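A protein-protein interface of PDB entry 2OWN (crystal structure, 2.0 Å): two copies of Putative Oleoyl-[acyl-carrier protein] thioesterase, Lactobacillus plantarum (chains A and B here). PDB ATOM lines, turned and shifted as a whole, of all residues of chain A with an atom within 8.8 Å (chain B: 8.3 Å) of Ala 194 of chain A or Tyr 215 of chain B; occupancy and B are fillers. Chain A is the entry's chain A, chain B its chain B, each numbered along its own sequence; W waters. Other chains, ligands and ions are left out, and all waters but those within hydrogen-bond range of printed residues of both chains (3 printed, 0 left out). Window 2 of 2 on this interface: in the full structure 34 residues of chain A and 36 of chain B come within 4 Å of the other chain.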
ATOM      1  N   ARG A  25      -6.207  -2.004   2.845  1.00  0.00           N
ATOM      2  CA  ARG A  25      -4.719  -1.997   2.764  1.00  0.00           C
ATOM      3  C   ARG A  25      -4.062  -2.556   1.471  1.00  0.00           C
ATOM      4  O   ARG A  25      -2.891  -2.272   1.236  1.00  0.00           O
ATOM      5  CB  ARG A  25      -4.071  -2.656   4.001  1.00  0.00           C
ATOM      6  CG  ARG A  25      -4.426  -4.125   4.251  1.00  0.00           C
ATOM      7  CD  ARG A  25      -3.634  -4.679   5.423  1.00  0.00           C
ATOM      8  NE  ARG A  25      -2.193  -4.773   5.142  1.00  0.00           N
ATOM      9  CZ  ARG A  25      -1.241  -5.173   6.001  1.00  0.00           C
ATOM     10  NH1 ARG A  25      -1.523  -5.528   7.272  1.00  0.00           N
ATOM     11  NH2 ARG A  25       0.031  -5.209   5.585  1.00  0.00           N
ATOM     12  N   THR A  26      -4.808  -3.333   0.673  1.00  0.00           N
ATOM     13  CA  THR A  26      -4.343  -3.878  -0.622  1.00  0.00           C
ATOM     14  C   THR A  26      -4.559  -2.902  -1.823  1.00  0.00           C
ATOM     15  O   THR A  26      -4.186  -3.254  -2.961  1.00  0.00           O
ATOM     16  CB  THR A  26      -5.036  -5.246  -0.960  1.00  0.00           C
ATOM     17  OG1 THR A  26      -6.421  -5.044  -1.256  1.00  0.00           O
ATOM     18  CG2 THR A  26      -4.893  -6.265   0.193  1.00  0.00           C
ATOM     19  N   ILE A 162     -15.620 -17.864  14.851  1.00  0.00           N
ATOM     20  CA  ILE A 162     -14.944 -16.630  15.245  1.00  0.00           C
ATOM     21  C   ILE A 162     -16.090 -15.702  15.621  1.00  0.00           C
ATOM     22  O   ILE A 162     -17.024 -15.536  14.820  1.00  0.00           O
ATOM     23  CB  ILE A 162     -14.139 -15.960  14.101  1.00  0.00           C
ATOM     24  CG1 ILE A 162     -13.116 -16.914  13.471  1.00  0.00           C
ATOM     25  CG2 ILE A 162     -13.423 -14.699  14.628  1.00  0.00           C
ATOM     26  CD1 ILE A 162     -12.473 -16.346  12.200  1.00  0.00           C
ATOM     27  N   LYS A 164     -16.827 -11.729  17.406  1.00  0.00           N
ATOM     28  CA  LYS A 164     -16.321 -10.403  17.813  1.00  0.00           C
ATOM     29  C   LYS A 164     -17.475  -9.419  18.054  1.00  0.00           C
ATOM     30  O   LYS A 164     -18.406  -9.381  17.226  1.00  0.00           O
ATOM     31  CB  LYS A 164     -15.389  -9.781  16.773  1.00  0.00           C
ATOM     32  CG  LYS A 164     -14.079 -10.515  16.501  1.00  0.00           C
ATOM     33  CD  LYS A 164     -13.204  -9.654  15.588  1.00  0.00           C
ATOM     34  CE  LYS A 164     -11.880 -10.296  15.226  1.00  0.00           C
ATOM     35  NZ  LYS A 164     -11.087  -9.385  14.351  1.00  0.00           N
ATOM     36  N   TYR A 166     -19.190  -5.618  18.224  1.00  0.00           N
ATOM     37  CA  TYR A 166     -19.090  -4.301  17.568  1.00  0.00           C
ATOM     38  C   TYR A 166     -20.230  -3.421  18.077  1.00  0.00           C
ATOM     39  O   TYR A 166     -21.358  -3.899  18.179  1.00  0.00           O
ATOM     40  CB  TYR A 166     -19.169  -4.385  16.039  1.00  0.00           C
ATOM     41  CG  TYR A 166     -18.093  -5.221  15.391  1.00  0.00           C
ATOM     42  CD1 TYR A 166     -16.864  -4.643  15.021  1.00  0.00           C
ATOM     43  CD2 TYR A 166     -18.281  -6.604  15.148  1.00  0.00           C
ATOM     44  CE1 TYR A 166     -15.832  -5.411  14.412  1.00  0.00           C
ATOM     45  CE2 TYR A 166     -17.252  -7.389  14.536  1.00  0.00           C
ATOM     46  CZ  TYR A 166     -16.035  -6.781  14.172  1.00  0.00           C
ATOM     47  OH  TYR A 166     -15.047  -7.528  13.588  1.00  0.00           O
ATOM     48  N   VAL A 189     -16.513  -8.548   7.568  1.00  0.00           N
ATOM     49  CA  VAL A 189     -15.149  -8.735   7.021  1.00  0.00           C
ATOM     50  C   VAL A 189     -14.088  -8.699   8.119  1.00  0.00           C
ATOM     51  O   VAL A 189     -13.185  -9.544   8.101  1.00  0.00           O
ATOM     52  CB  VAL A 189     -14.826  -7.722   5.872  1.00  0.00           C
ATOM     53  CG1 VAL A 189     -13.401  -7.908   5.320  1.00  0.00           C
ATOM     54  CG2 VAL A 189     -15.837  -7.868   4.739  1.00  0.00           C
ATOM     55  N   ASP A 190     -14.200  -7.745   9.062  1.00  0.00           N
ATOM     56  CA  ASP A 190     -13.245  -7.624  10.201  1.00  0.00           C
ATOM     57  C   ASP A 190     -13.264  -8.847  11.155  1.00  0.00           C
ATOM     58  O   ASP A 190     -12.282  -9.062  11.877  1.00  0.00           O
ATOM     59  CB  ASP A 190     -13.437  -6.308  10.981  1.00  0.00           C
ATOM     60  CG  ASP A 190     -12.369  -6.080  12.032  1.00  0.00           C
ATOM     61  OD1 ASP A 190     -11.175  -6.056  11.664  1.00  0.00           O
ATOM     62  OD2 ASP A 190     -12.728  -5.949  13.210  1.00  0.00           O
ATOM     63  N   THR A 191     -14.363  -9.621  11.169  1.00  0.00           N
ATOM     64  CA  THR A 191     -14.458 -10.888  11.947  1.00  0.00           C
ATOM     65  C   THR A 191     -13.366 -11.886  11.489  1.00  0.00           C
ATOM     66  O   THR A 191     -12.807 -12.602  12.317  1.00  0.00           O
ATOM     67  CB  THR A 191     -15.849 -11.566  11.822  1.00  0.00           C
ATOM     68  OG1 THR A 191     -16.886 -10.604  12.088  1.00  0.00           O
ATOM     69  CG2 THR A 191     -15.978 -12.743  12.789  1.00  0.00           C
ATOM     70  N   LEU A 192     -13.083 -11.913  10.178  1.00  0.00           N
ATOM     71  CA  LEU A 192     -12.044 -12.769   9.583  1.00  0.00           C
ATOM     72  C   LEU A 192     -10.650 -12.149   9.885  1.00  0.00           C
ATOM     73  O   LEU A 192     -10.527 -10.910   9.877  1.00  0.00           O
ATOM     74  CB  LEU A 192     -12.263 -12.920   8.067  1.00  0.00           C
ATOM     75  CG  LEU A 192     -13.593 -13.566   7.641  1.00  0.00           C
ATOM     76  CD1 LEU A 192     -13.877 -13.347   6.166  1.00  0.00           C
ATOM     77  CD2 LEU A 192     -13.599 -15.052   7.994  1.00  0.00           C
ATOM     78  N   PRO A 193      -9.607 -12.984  10.133  1.00  0.00           N
ATOM     79  CA  PRO A 193      -8.264 -12.439  10.437  1.00  0.00           C
ATOM     80  C   PRO A 193      -7.583 -11.832   9.200  1.00  0.00           C
ATOM     81  O   PRO A 193      -7.870 -12.268   8.070  1.00  0.00           O
ATOM     82  CB  PRO A 193      -7.500 -13.672  10.926  1.00  0.00           C
ATOM     83  CG  PRO A 193      -8.096 -14.774  10.157  1.00  0.00           C
ATOM     84  CD  PRO A 193      -9.564 -14.460  10.102  1.00  0.00           C
ATOM     85  N   ALA A 194      -6.710 -10.841   9.427  1.00  0.00           N
ATOM     86  CA  ALA A 194      -5.942 -10.142   8.354  1.00  0.00           C
ATOM     87  C   ALA A 194      -5.206 -11.097   7.396  1.00  0.00           C
ATOM     88  O   ALA A 194      -5.171 -10.830   6.199  1.00  0.00           O
ATOM     89  CB  ALA A 194      -4.948  -9.120   8.946  1.00  0.00           C
ATOM     90  N   THR A 195      -4.651 -12.196   7.943  1.00  0.00           N
ATOM     91  CA  THR A 195      -3.952 -13.258   7.176  1.00  0.00           C
ATOM     92  C   THR A 195      -4.886 -13.910   6.155  1.00  0.00           C
ATOM     93  O   THR A 195      -4.457 -14.141   5.034  1.00  0.00           O
ATOM     94  CB  THR A 195      -3.358 -14.371   8.069  1.00  0.00           C
ATOM     95  OG1 THR A 195      -4.393 -14.892   8.913  1.00  0.00           O
ATOM     96  CG2 THR A 195      -2.219 -13.829   8.933  1.00  0.00           C
ATOM     97  N   PHE A 196      -6.135 -14.200   6.561  1.00  0.00           N
ATOM     98  CA  PHE A 196      -7.174 -14.765   5.664  1.00  0.00           C
ATOM     99  C   PHE A 196      -7.534 -13.743   4.574  1.00  0.00           C
ATOM    100  O   PHE A 196      -7.578 -14.102   3.392  1.00  0.00           O
ATOM    101  CB  PHE A 196      -8.452 -15.206   6.427  1.00  0.00           C
ATOM    102  CG  PHE A 196      -9.510 -15.852   5.547  1.00  0.00           C
ATOM    103  CD1 PHE A 196     -10.465 -15.057   4.868  1.00  0.00           C
ATOM    104  CD2 PHE A 196      -9.556 -17.250   5.383  1.00  0.00           C
ATOM    105  CE1 PHE A 196     -11.435 -15.643   4.008  1.00  0.00           C
ATOM    106  CE2 PHE A 196     -10.544 -17.856   4.548  1.00  0.00           C
ATOM    107  CZ  PHE A 196     -11.488 -17.044   3.858  1.00  0.00           C
ATOM    108  N   LEU A 197      -7.789 -12.498   4.994  1.00  0.00           N
ATOM    109  CA  LEU A 197      -8.173 -11.394   4.087  1.00  0.00           C
ATOM    110  C   LEU A 197      -7.105 -11.007   3.048  1.00  0.00           C
ATOM    111  O   LEU A 197      -7.468 -10.650   1.925  1.00  0.00           O
ATOM    112  CB  LEU A 197      -8.618 -10.144   4.888  1.00  0.00           C
ATOM    113  CG  LEU A 197      -9.836 -10.326   5.807  1.00  0.00           C
ATOM    114  CD1 LEU A 197     -10.043  -9.115   6.722  1.00  0.00           C
ATOM    115  CD2 LEU A 197     -11.104 -10.631   4.980  1.00  0.00           C
ATOM    116  N   LEU A 198      -5.819 -11.097   3.412  1.00  0.00           N
ATOM    117  CA  LEU A 198      -4.702 -10.760   2.496  1.00  0.00           C
ATOM    118  C   LEU A 198      -4.345 -11.842   1.464  1.00  0.00           C
ATOM    119  O   LEU A 198      -3.704 -11.486   0.465  1.00  0.00           O
ATOM    120  CB  LEU A 198      -3.450 -10.302   3.282  1.00  0.00           C
ATOM    121  CG  LEU A 198      -3.582  -8.950   4.015  1.00  0.00           C
ATOM    122  CD1 LEU A 198      -2.430  -8.746   4.991  1.00  0.00           C
ATOM    123  CD2 LEU A 198      -3.683  -7.770   3.041  1.00  0.00           C
ATOM    124  N   GLN A 199      -4.720 -13.116   1.687  1.00  0.00           N
ATOM    125  CA  GLN A 199      -4.454 -14.220   0.719  1.00  0.00           C
ATOM    126  C   GLN A 199      -5.733 -14.867   0.133  1.00  0.00           C
ATOM    127  O   GLN A 199      -5.735 -16.050  -0.240  1.00  0.00           O
ATOM    128  CB  GLN A 199      -3.474 -15.243   1.316  1.00  0.00           C
ATOM    129  CG  GLN A 199      -3.971 -16.155   2.437  1.00  0.00           C
ATOM    130  CD  GLN A 199      -2.821 -16.911   3.134  1.00  0.00           C
ATOM    131  OE1 GLN A 199      -1.789 -17.208   2.519  1.00  0.00           O
ATOM    132  NE2 GLN A 199      -3.009 -17.240   4.406  1.00  0.00           N
ATOM    133  N   HIS A 200      -6.795 -14.056   0.018  1.00  0.00           N
ATOM    134  CA  HIS A 200      -8.098 -14.440  -0.568  1.00  0.00           C
ATOM    135  C   HIS A 200      -8.763 -13.240  -1.254  1.00  0.00           C
ATOM    136  O   HIS A 200      -8.734 -12.128  -0.704  1.00  0.00           O
ATOM    137  CB  HIS A 200      -9.082 -15.018   0.461  1.00  0.00           C
ATOM    138  CG  HIS A 200      -8.688 -16.350   1.013  1.00  0.00           C
ATOM    139  ND1 HIS A 200      -7.905 -16.491   2.139  1.00  0.00           N
ATOM    140  CD2 HIS A 200      -8.983 -17.606   0.600  1.00  0.00           C
ATOM    141  CE1 HIS A 200      -7.720 -17.775   2.384  1.00  0.00           C
ATOM    142  NE2 HIS A 200      -8.362 -18.474   1.466  1.00  0.00           N
ATOM    143  N   HIS B 167     -12.039  -1.000  19.045  1.00  0.00           N
ATOM    144  CA  HIS B 167     -11.093  -1.975  18.497  1.00  0.00           C
ATOM    145  C   HIS B 167     -10.719  -1.483  17.102  1.00  0.00           C
ATOM    146  O   HIS B 167     -11.595  -1.013  16.355  1.00  0.00           O
ATOM    147  CB  HIS B 167     -11.712  -3.363  18.458  1.00  0.00           C
ATOM    148  CG  HIS B 167     -12.076  -3.886  19.812  1.00  0.00           C
ATOM    149  ND1 HIS B 167     -13.266  -3.575  20.433  1.00  0.00           N
ATOM    150  CD2 HIS B 167     -11.402  -4.689  20.667  1.00  0.00           C
ATOM    151  CE1 HIS B 167     -13.309  -4.166  21.615  1.00  0.00           C
ATOM    152  NE2 HIS B 167     -12.190  -4.849  21.780  1.00  0.00           N
ATOM    153  N   VAL B 168      -9.428  -1.585  16.761  1.00  0.00           N
ATOM    154  CA  VAL B 168      -8.904  -1.161  15.453  1.00  0.00           C
ATOM    155  C   VAL B 168      -9.287  -2.272  14.462  1.00  0.00           C
ATOM    156  O   VAL B 168      -8.933  -3.433  14.677  1.00  0.00           O
ATOM    157  CB  VAL B 168      -7.378  -0.917  15.459  1.00  0.00           C
ATOM    158  CG1 VAL B 168      -6.875  -0.459  14.084  1.00  0.00           C
ATOM    159  CG2 VAL B 168      -7.027   0.122  16.500  1.00  0.00           C
ATOM    160  N   ARG B 169     -10.011  -1.897  13.407  1.00  0.00           N
ATOM    161  CA  ARG B 169     -10.501  -2.827  12.370  1.00  0.00           C
ATOM    162  C   ARG B 169      -9.573  -2.946  11.184  1.00  0.00           C
ATOM    163  O   ARG B 169      -8.678  -2.116  11.010  1.00  0.00           O
ATOM    164  CB  ARG B 169     -11.849  -2.364  11.842  1.00  0.00           C
ATOM    165  CG  ARG B 169     -12.894  -2.363  12.874  1.00  0.00           C
ATOM    166  CD  ARG B 169     -14.109  -1.699  12.366  1.00  0.00           C
ATOM    167  NE  ARG B 169     -15.071  -1.648  13.443  1.00  0.00           N
ATOM    168  CZ  ARG B 169     -16.132  -0.850  13.506  1.00  0.00           C
ATOM    169  NH1 ARG B 169     -16.456   0.020  12.548  1.00  0.00           N
ATOM    170  NH2 ARG B 169     -16.882  -0.932  14.593  1.00  0.00           N
ATOM    171  N   PHE B 170      -9.826  -3.976  10.363  1.00  0.00           N
ATOM    172  CA  PHE B 170      -9.064  -4.237   9.136  1.00  0.00           C
ATOM    173  C   PHE B 170      -9.180  -3.030   8.185  1.00  0.00           C
ATOM    174  O   PHE B 170      -8.139  -2.530   7.757  1.00  0.00           O
ATOM    175  CB  PHE B 170      -9.491  -5.541   8.446  1.00  0.00           C
ATOM    176  CG  PHE B 170      -8.709  -5.847   7.207  1.00  0.00           C
ATOM    177  CD1 PHE B 170      -7.401  -6.355   7.308  1.00  0.00           C
ATOM    178  CD2 PHE B 170      -9.265  -5.624   5.927  1.00  0.00           C
ATOM    179  CE1 PHE B 170      -6.639  -6.642   6.146  1.00  0.00           C
ATOM    180  CE2 PHE B 170      -8.524  -5.907   4.749  1.00  0.00           C
ATOM    181  CZ  PHE B 170      -7.204  -6.419   4.855  1.00  0.00           C
ATOM    182  N   PHE B 171     -10.406  -2.520   7.961  1.00  0.00           N
ATOM    183  CA  PHE B 171     -10.615  -1.340   7.074  1.00  0.00           C
ATOM    184  C   PHE B 171     -10.029  -0.004   7.596  1.00  0.00           C
ATOM    185  O   PHE B 171      -9.968   0.945   6.813  1.00  0.00           O
ATOM    186  CB  PHE B 171     -12.085  -1.145   6.605  1.00  0.00           C
ATOM    187  CG  PHE B 171     -12.711  -2.348   5.896  1.00  0.00           C
ATOM    188  CD1 PHE B 171     -11.966  -3.217   5.046  1.00  0.00           C
ATOM    189  CD2 PHE B 171     -14.117  -2.505   5.935  1.00  0.00           C
ATOM    190  CE1 PHE B 171     -12.594  -4.311   4.371  1.00  0.00           C
ATOM    191  CE2 PHE B 171     -14.766  -3.577   5.250  1.00  0.00           C
ATOM    192  CZ  PHE B 171     -14.000  -4.485   4.465  1.00  0.00           C
ATOM    193  N   ASP B 172      -9.633   0.082   8.878  1.00  0.00           N
ATOM    194  CA  ASP B 172      -8.948   1.277   9.420  1.00  0.00           C
ATOM    195  C   ASP B 172      -7.514   1.441   8.847  1.00  0.00           C
ATOM    196  O   ASP B 172      -7.016   2.570   8.811  1.00  0.00           O
ATOM    197  CB  ASP B 172      -8.890   1.280  10.960  1.00  0.00           C
ATOM    198  CG  ASP B 172     -10.264   1.354  11.611  1.00  0.00           C
ATOM    199  OD1 ASP B 172     -11.165   2.019  11.079  1.00  0.00           O
ATOM    200  OD2 ASP B 172     -10.423   0.786  12.700  1.00  0.00           O
ATOM    201  N   ILE B 173      -6.877   0.338   8.415  1.00  0.00           N
ATOM    202  CA  ILE B 173      -5.525   0.329   7.824  1.00  0.00           C
ATOM    203  C   ILE B 173      -5.716   0.612   6.321  1.00  0.00           C
ATOM    204  O   ILE B 173      -6.154  -0.274   5.592  1.00  0.00           O
ATOM    205  CB  ILE B 173      -4.741  -0.999   8.093  1.00  0.00           C
ATOM    206  CG1 ILE B 173      -4.357  -1.159   9.576  1.00  0.00           C
ATOM    207  CG2 ILE B 173      -3.417  -1.038   7.323  1.00  0.00           C
ATOM    208  CD1 ILE B 173      -5.483  -1.295  10.589  1.00  0.00           C
ATOM    209  N   ARG B 177      -0.392   0.539   4.388  1.00  0.00           N
ATOM    210  CA  ARG B 177      -0.158  -0.439   5.489  1.00  0.00           C
ATOM    211  C   ARG B 177      -0.052   0.186   6.919  1.00  0.00           C
ATOM    212  O   ARG B 177       0.692  -0.315   7.782  1.00  0.00           O
ATOM    213  CB  ARG B 177       1.045  -1.360   5.146  1.00  0.00           C
ATOM    214  CG  ARG B 177       0.928  -2.092   3.801  1.00  0.00           C
ATOM    215  CD  ARG B 177       2.147  -2.970   3.538  1.00  0.00           C
ATOM    216  N   HIS B 178      -0.801   1.275   7.146  1.00  0.00           N
ATOM    217  CA  HIS B 178      -0.860   2.012   8.436  1.00  0.00           C
ATOM    218  C   HIS B 178      -2.296   2.470   8.742  1.00  0.00           C
ATOM    219  O   HIS B 178      -3.062   2.718   7.800  1.00  0.00           O
ATOM    220  CB  HIS B 178       0.058   3.244   8.429  1.00  0.00           C
ATOM    221  CG  HIS B 178       1.504   2.935   8.188  1.00  0.00           C
ATOM    222  ND1 HIS B 178       2.093   3.055   6.947  1.00  0.00           N
ATOM    223  CD2 HIS B 178       2.473   2.490   9.022  1.00  0.00           C
ATOM    224  CE1 HIS B 178       3.366   2.711   7.031  1.00  0.00           C
ATOM    225  NE2 HIS B 178       3.621   2.364   8.279  1.00  0.00           N
ATOM    226  N   VAL B 179      -2.634   2.600  10.035  1.00  0.00           N
ATOM    227  CA  VAL B 179      -3.977   3.044  10.483  1.00  0.00           C
ATOM    228  C   VAL B 179      -4.161   4.530  10.146  1.00  0.00           C
ATOM    229  O   VAL B 179      -3.467   5.374  10.727  1.00  0.00           O
ATOM    230  CB  VAL B 179      -4.235   2.799  12.002  1.00  0.00           C
ATOM    231  CG1 VAL B 179      -5.586   3.372  12.474  1.00  0.00           C
ATOM    232  CG2 VAL B 179      -4.187   1.317  12.295  1.00  0.00           C
ATOM    233  N   GLU B 212       1.246   6.207  17.131  1.00  0.00           N
ATOM    234  CA  GLU B 212       0.393   5.546  16.126  1.00  0.00           C
ATOM    235  C   GLU B 212      -0.255   4.291  16.723  1.00  0.00           C
ATOM    236  O   GLU B 212       0.362   3.602  17.547  1.00  0.00           O
ATOM    237  CB  GLU B 212       1.174   5.165  14.864  1.00  0.00           C
ATOM    238  CG  GLU B 212       1.755   6.352  14.104  1.00  0.00           C
ATOM    239  N   VAL B 213      -1.501   4.035  16.321  1.00  0.00           N
ATOM    240  CA  VAL B 213      -2.283   2.871  16.755  1.00  0.00           C
ATOM    241  C   VAL B 213      -2.134   1.815  15.650  1.00  0.00           C
ATOM    242  O   VAL B 213      -2.111   2.162  14.466  1.00  0.00           O
ATOM    243  CB  VAL B 213      -3.759   3.228  16.994  1.00  0.00           C
ATOM    244  CG1 VAL B 213      -4.512   2.028  17.520  1.00  0.00           C
ATOM    245  CG2 VAL B 213      -3.880   4.375  17.997  1.00  0.00           C
ATOM    246  N   LYS B 214      -2.010   0.547  16.051  1.00  0.00           N
ATOM    247  CA  LYS B 214      -1.853  -0.596  15.140  1.00  0.00           C
ATOM    248  C   LYS B 214      -3.068  -1.529  15.161  1.00  0.00           C
ATOM    249  O   LYS B 214      -3.925  -1.441  16.057  1.00  0.00           O
ATOM    250  CB  LYS B 214      -0.584  -1.380  15.493  1.00  0.00           C
ATOM    251  CG  LYS B 214       0.708  -0.577  15.353  1.00  0.00           C
ATOM    252  CD  LYS B 214       1.937  -1.422  15.680  1.00  0.00           C
ATOM    253  N   TYR B 215      -3.126  -2.406  14.148  1.00  0.00           N
ATOM    254  CA  TYR B 215      -4.181  -3.431  13.977  1.00  0.00           C
ATOM    255  C   TYR B 215      -4.106  -4.430  15.140  1.00  0.00           C
ATOM    256  O   TYR B 215      -3.002  -4.806  15.568  1.00  0.00           O
ATOM    257  CB  TYR B 215      -4.046  -4.141  12.611  1.00  0.00           C
ATOM    258  CG  TYR B 215      -4.974  -5.318  12.372  1.00  0.00           C
ATOM    259  CD1 TYR B 215      -6.328  -5.125  11.991  1.00  0.00           C
ATOM    260  CD2 TYR B 215      -4.495  -6.647  12.499  1.00  0.00           C
ATOM    261  CE1 TYR B 215      -7.199  -6.250  11.757  1.00  0.00           C
ATOM    262  CE2 TYR B 215      -5.347  -7.772  12.266  1.00  0.00           C
ATOM    263  CZ  TYR B 215      -6.691  -7.565  11.895  1.00  0.00           C
ATOM    264  OH  TYR B 215      -7.483  -8.661  11.683  1.00  0.00           O
ATOM    265  N   GLY B 216      -5.278  -4.813  15.659  1.00  0.00           N
ATOM    266  CA  GLY B 216      -5.388  -5.728  16.809  1.00  0.00           C
ATOM    267  C   GLY B 216      -5.419  -5.063  18.188  1.00  0.00           C
ATOM    268  O   GLY B 216      -5.820  -5.726  19.155  1.00  0.00           O
ATOM    269  N   GLN B 217      -4.992  -3.792  18.294  1.00  0.00           N
ATOM    270  CA  GLN B 217      -4.996  -3.039  19.558  1.00  0.00           C
ATOM    271  C   GLN B 217      -6.399  -2.501  19.847  1.00  0.00           C
ATOM    272  O   GLN B 217      -7.165  -2.191  18.912  1.00  0.00           O
ATOM    273  CB  GLN B 217      -4.005  -1.862  19.542  1.00  0.00           C
ATOM    274  CG  GLN B 217      -2.536  -2.267  19.450  1.00  0.00           C
ATOM    275  CD  GLN B 217      -1.577  -1.071  19.450  1.00  0.00           C
ATOM    276  OE1 GLN B 217      -1.834  -0.042  18.822  1.00  0.00           O
ATOM    277  NE2 GLN B 217      -0.446  -1.228  20.121  1.00  0.00           N
ATOM    278  N   THR B 218      -6.720  -2.417  21.141  1.00  0.00           N
ATOM    279  CA  THR B 218      -7.983  -1.890  21.645  1.00  0.00           C
ATOM    280  C   THR B 218      -7.623  -0.512  22.204  1.00  0.00           C
ATOM    281  O   THR B 218      -6.795  -0.424  23.126  1.00  0.00           O
ATOM    282  CB  THR B 218      -8.596  -2.764  22.758  1.00  0.00           C
ATOM    283  OG1 THR B 218      -8.743  -4.111  22.291  1.00  0.00           O
ATOM    284  CG2 THR B 218      -9.967  -2.213  23.194  1.00  0.00           C
HETATM  285  O   HOH W   1      -9.881  -8.348  10.674  1.00  0.00           O
HETATM  286  O   HOH W   2      -7.473  -2.418   5.237  1.00  0.00           O
HETATM  287  O   HOH W   3      -8.889 -10.894  13.639  1.00  0.00           O
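No position is printed for both chains. Of the 10 pairs that touch across the chains among the printed residues, none has its exchanged pair printed and touching as well.
Water W2 lies within hydrogen-bond range of O of Ile 173 of chain B, O of Phe 170 of chain B and N of Arg 25 of chain A. Water W1 lies within hydrogen-bond range of the side-chain hydroxyl (OH) of Tyr 215 of chain B, the backbone carbonyl oxygen (O) of Leu 192 of chain A and the backbone carbonyl oxygen (O) of Asp 190 of chain A. Water W3 bridges NZ of Lys 164 of chain A and OH of Tyr 215 of chain B.
The backbone NH (N) of Arg 25 of chain A sits at hydrogen-bond distance from the backbone carbonyl oxygen (O) of Ile 173 of chain B, 3.2 Å away. N of Phe 170 of chain B lies within hydrogen-bond range of OD1 of Asp 190 of chain A (2.8 Å). The backbone NH (N) of Ala 194 of chain A lies within hydrogen-bond range of the side-chain hydroxyl (OH) of Tyr 215 of chain B (3.2 Å).
Of the printed residues of chain B, Val 189 of chain A touches Phe 171. Of the printed residues of chain B, Asp 190 of chain A touches Arg 169 (3.4 Å), Phe 170 (2.8 Å) and Tyr 215 (3.98 Å). Ala 194 of chain A touches one residue of chain B. Thr 195 of chain A touches none of the printed residues of chain B. Printed residues of chain A within 4 Å of Arg 169 of chain B: Tyr 166 (3.7 Å) and Asp 190 (3.4 Å). Of the printed residues of chain A, Phe 171 of chain B touches Val 189. Printed residues of chain A within 4 Å of Arg 177 of chain B: Arg 25. Printed residues of chain A within 4 Å of Tyr 215 of chain B: Asp 190 (3.98 Å) and Ala 194 (3.2 Å). No residue of chain A comes within 4 Å of Gly 216 of chain B. The nearest residue of chain B that does not touch Ala 194 of chain A is Phe 170 of chain B (4.04 Å). The nearest printed residue of chain B that does not touch Arg 25 of chain A is His 178 of chain B (6.0 Å).
Hydrophobic or aromatic side chains of chain B within 4 Å of the printed part of chain A: Phe 170, Phe 171, Ile 173 and Tyr 215. Printed residues of chain A that touch a printed residue of chain B: Arg 25, Tyr 166, Val 189, Asp 190, Ala 194 and Leu 197. Hydrophobic or aromatic side chains of chain A within 4 Å of the printed part of chain B: Tyr 166, Val 189, Ala 194 and Leu 197. Among the printed residues, 10 pairs touch across the chains. Among the printed residues, no Asp or Glu carboxylate lies within 4 Å of a Lys or Arg side-chain nitrogen of the other chain.
CZ of Phe 170 of chain B touches CG of Arg 25 of chain A, 3.7 Å away. Arg 25 of chain A touches Arg 177 of chain B (NH2 to CD, 3.7 Å). Arg 169 of chain B touches Tyr 166 of chain A (NH2 to CD1, 3.7 Å). Val 189 of chain A touches Phe 171 of chain B. Arg 169 of chain B touches Asp 190 of chain A. OD1 of Asp 190 of chain A touches CE1 of Tyr 215 of chain B, 3.98 Å away. Leu 197 of chain A touches Phe 170 of chain B (CD1 to CG, 3.6 Å).
The side-chain amino group (NZ) of Lys 164 of chain A lies within salt-bridge range of the side-chain carboxylate (OD2) of Asp 190 of chain A. OH of Tyr 166 of chain A sits at hydrogen-bond distance from OD2 of Asp 190 of chain A (2.8 Å). The backbone NH of Thr 191 of chain A is in hydrogen-bond range of the side-chain hydroxyl of Tyr 166 of chain A, at 3.3 Å. The backbone NH (N) of Arg 169 of chain B is in hydrogen-bond range of the side-chain carboxylate (OD2) of Asp 172 of chain B (2.8 Å).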
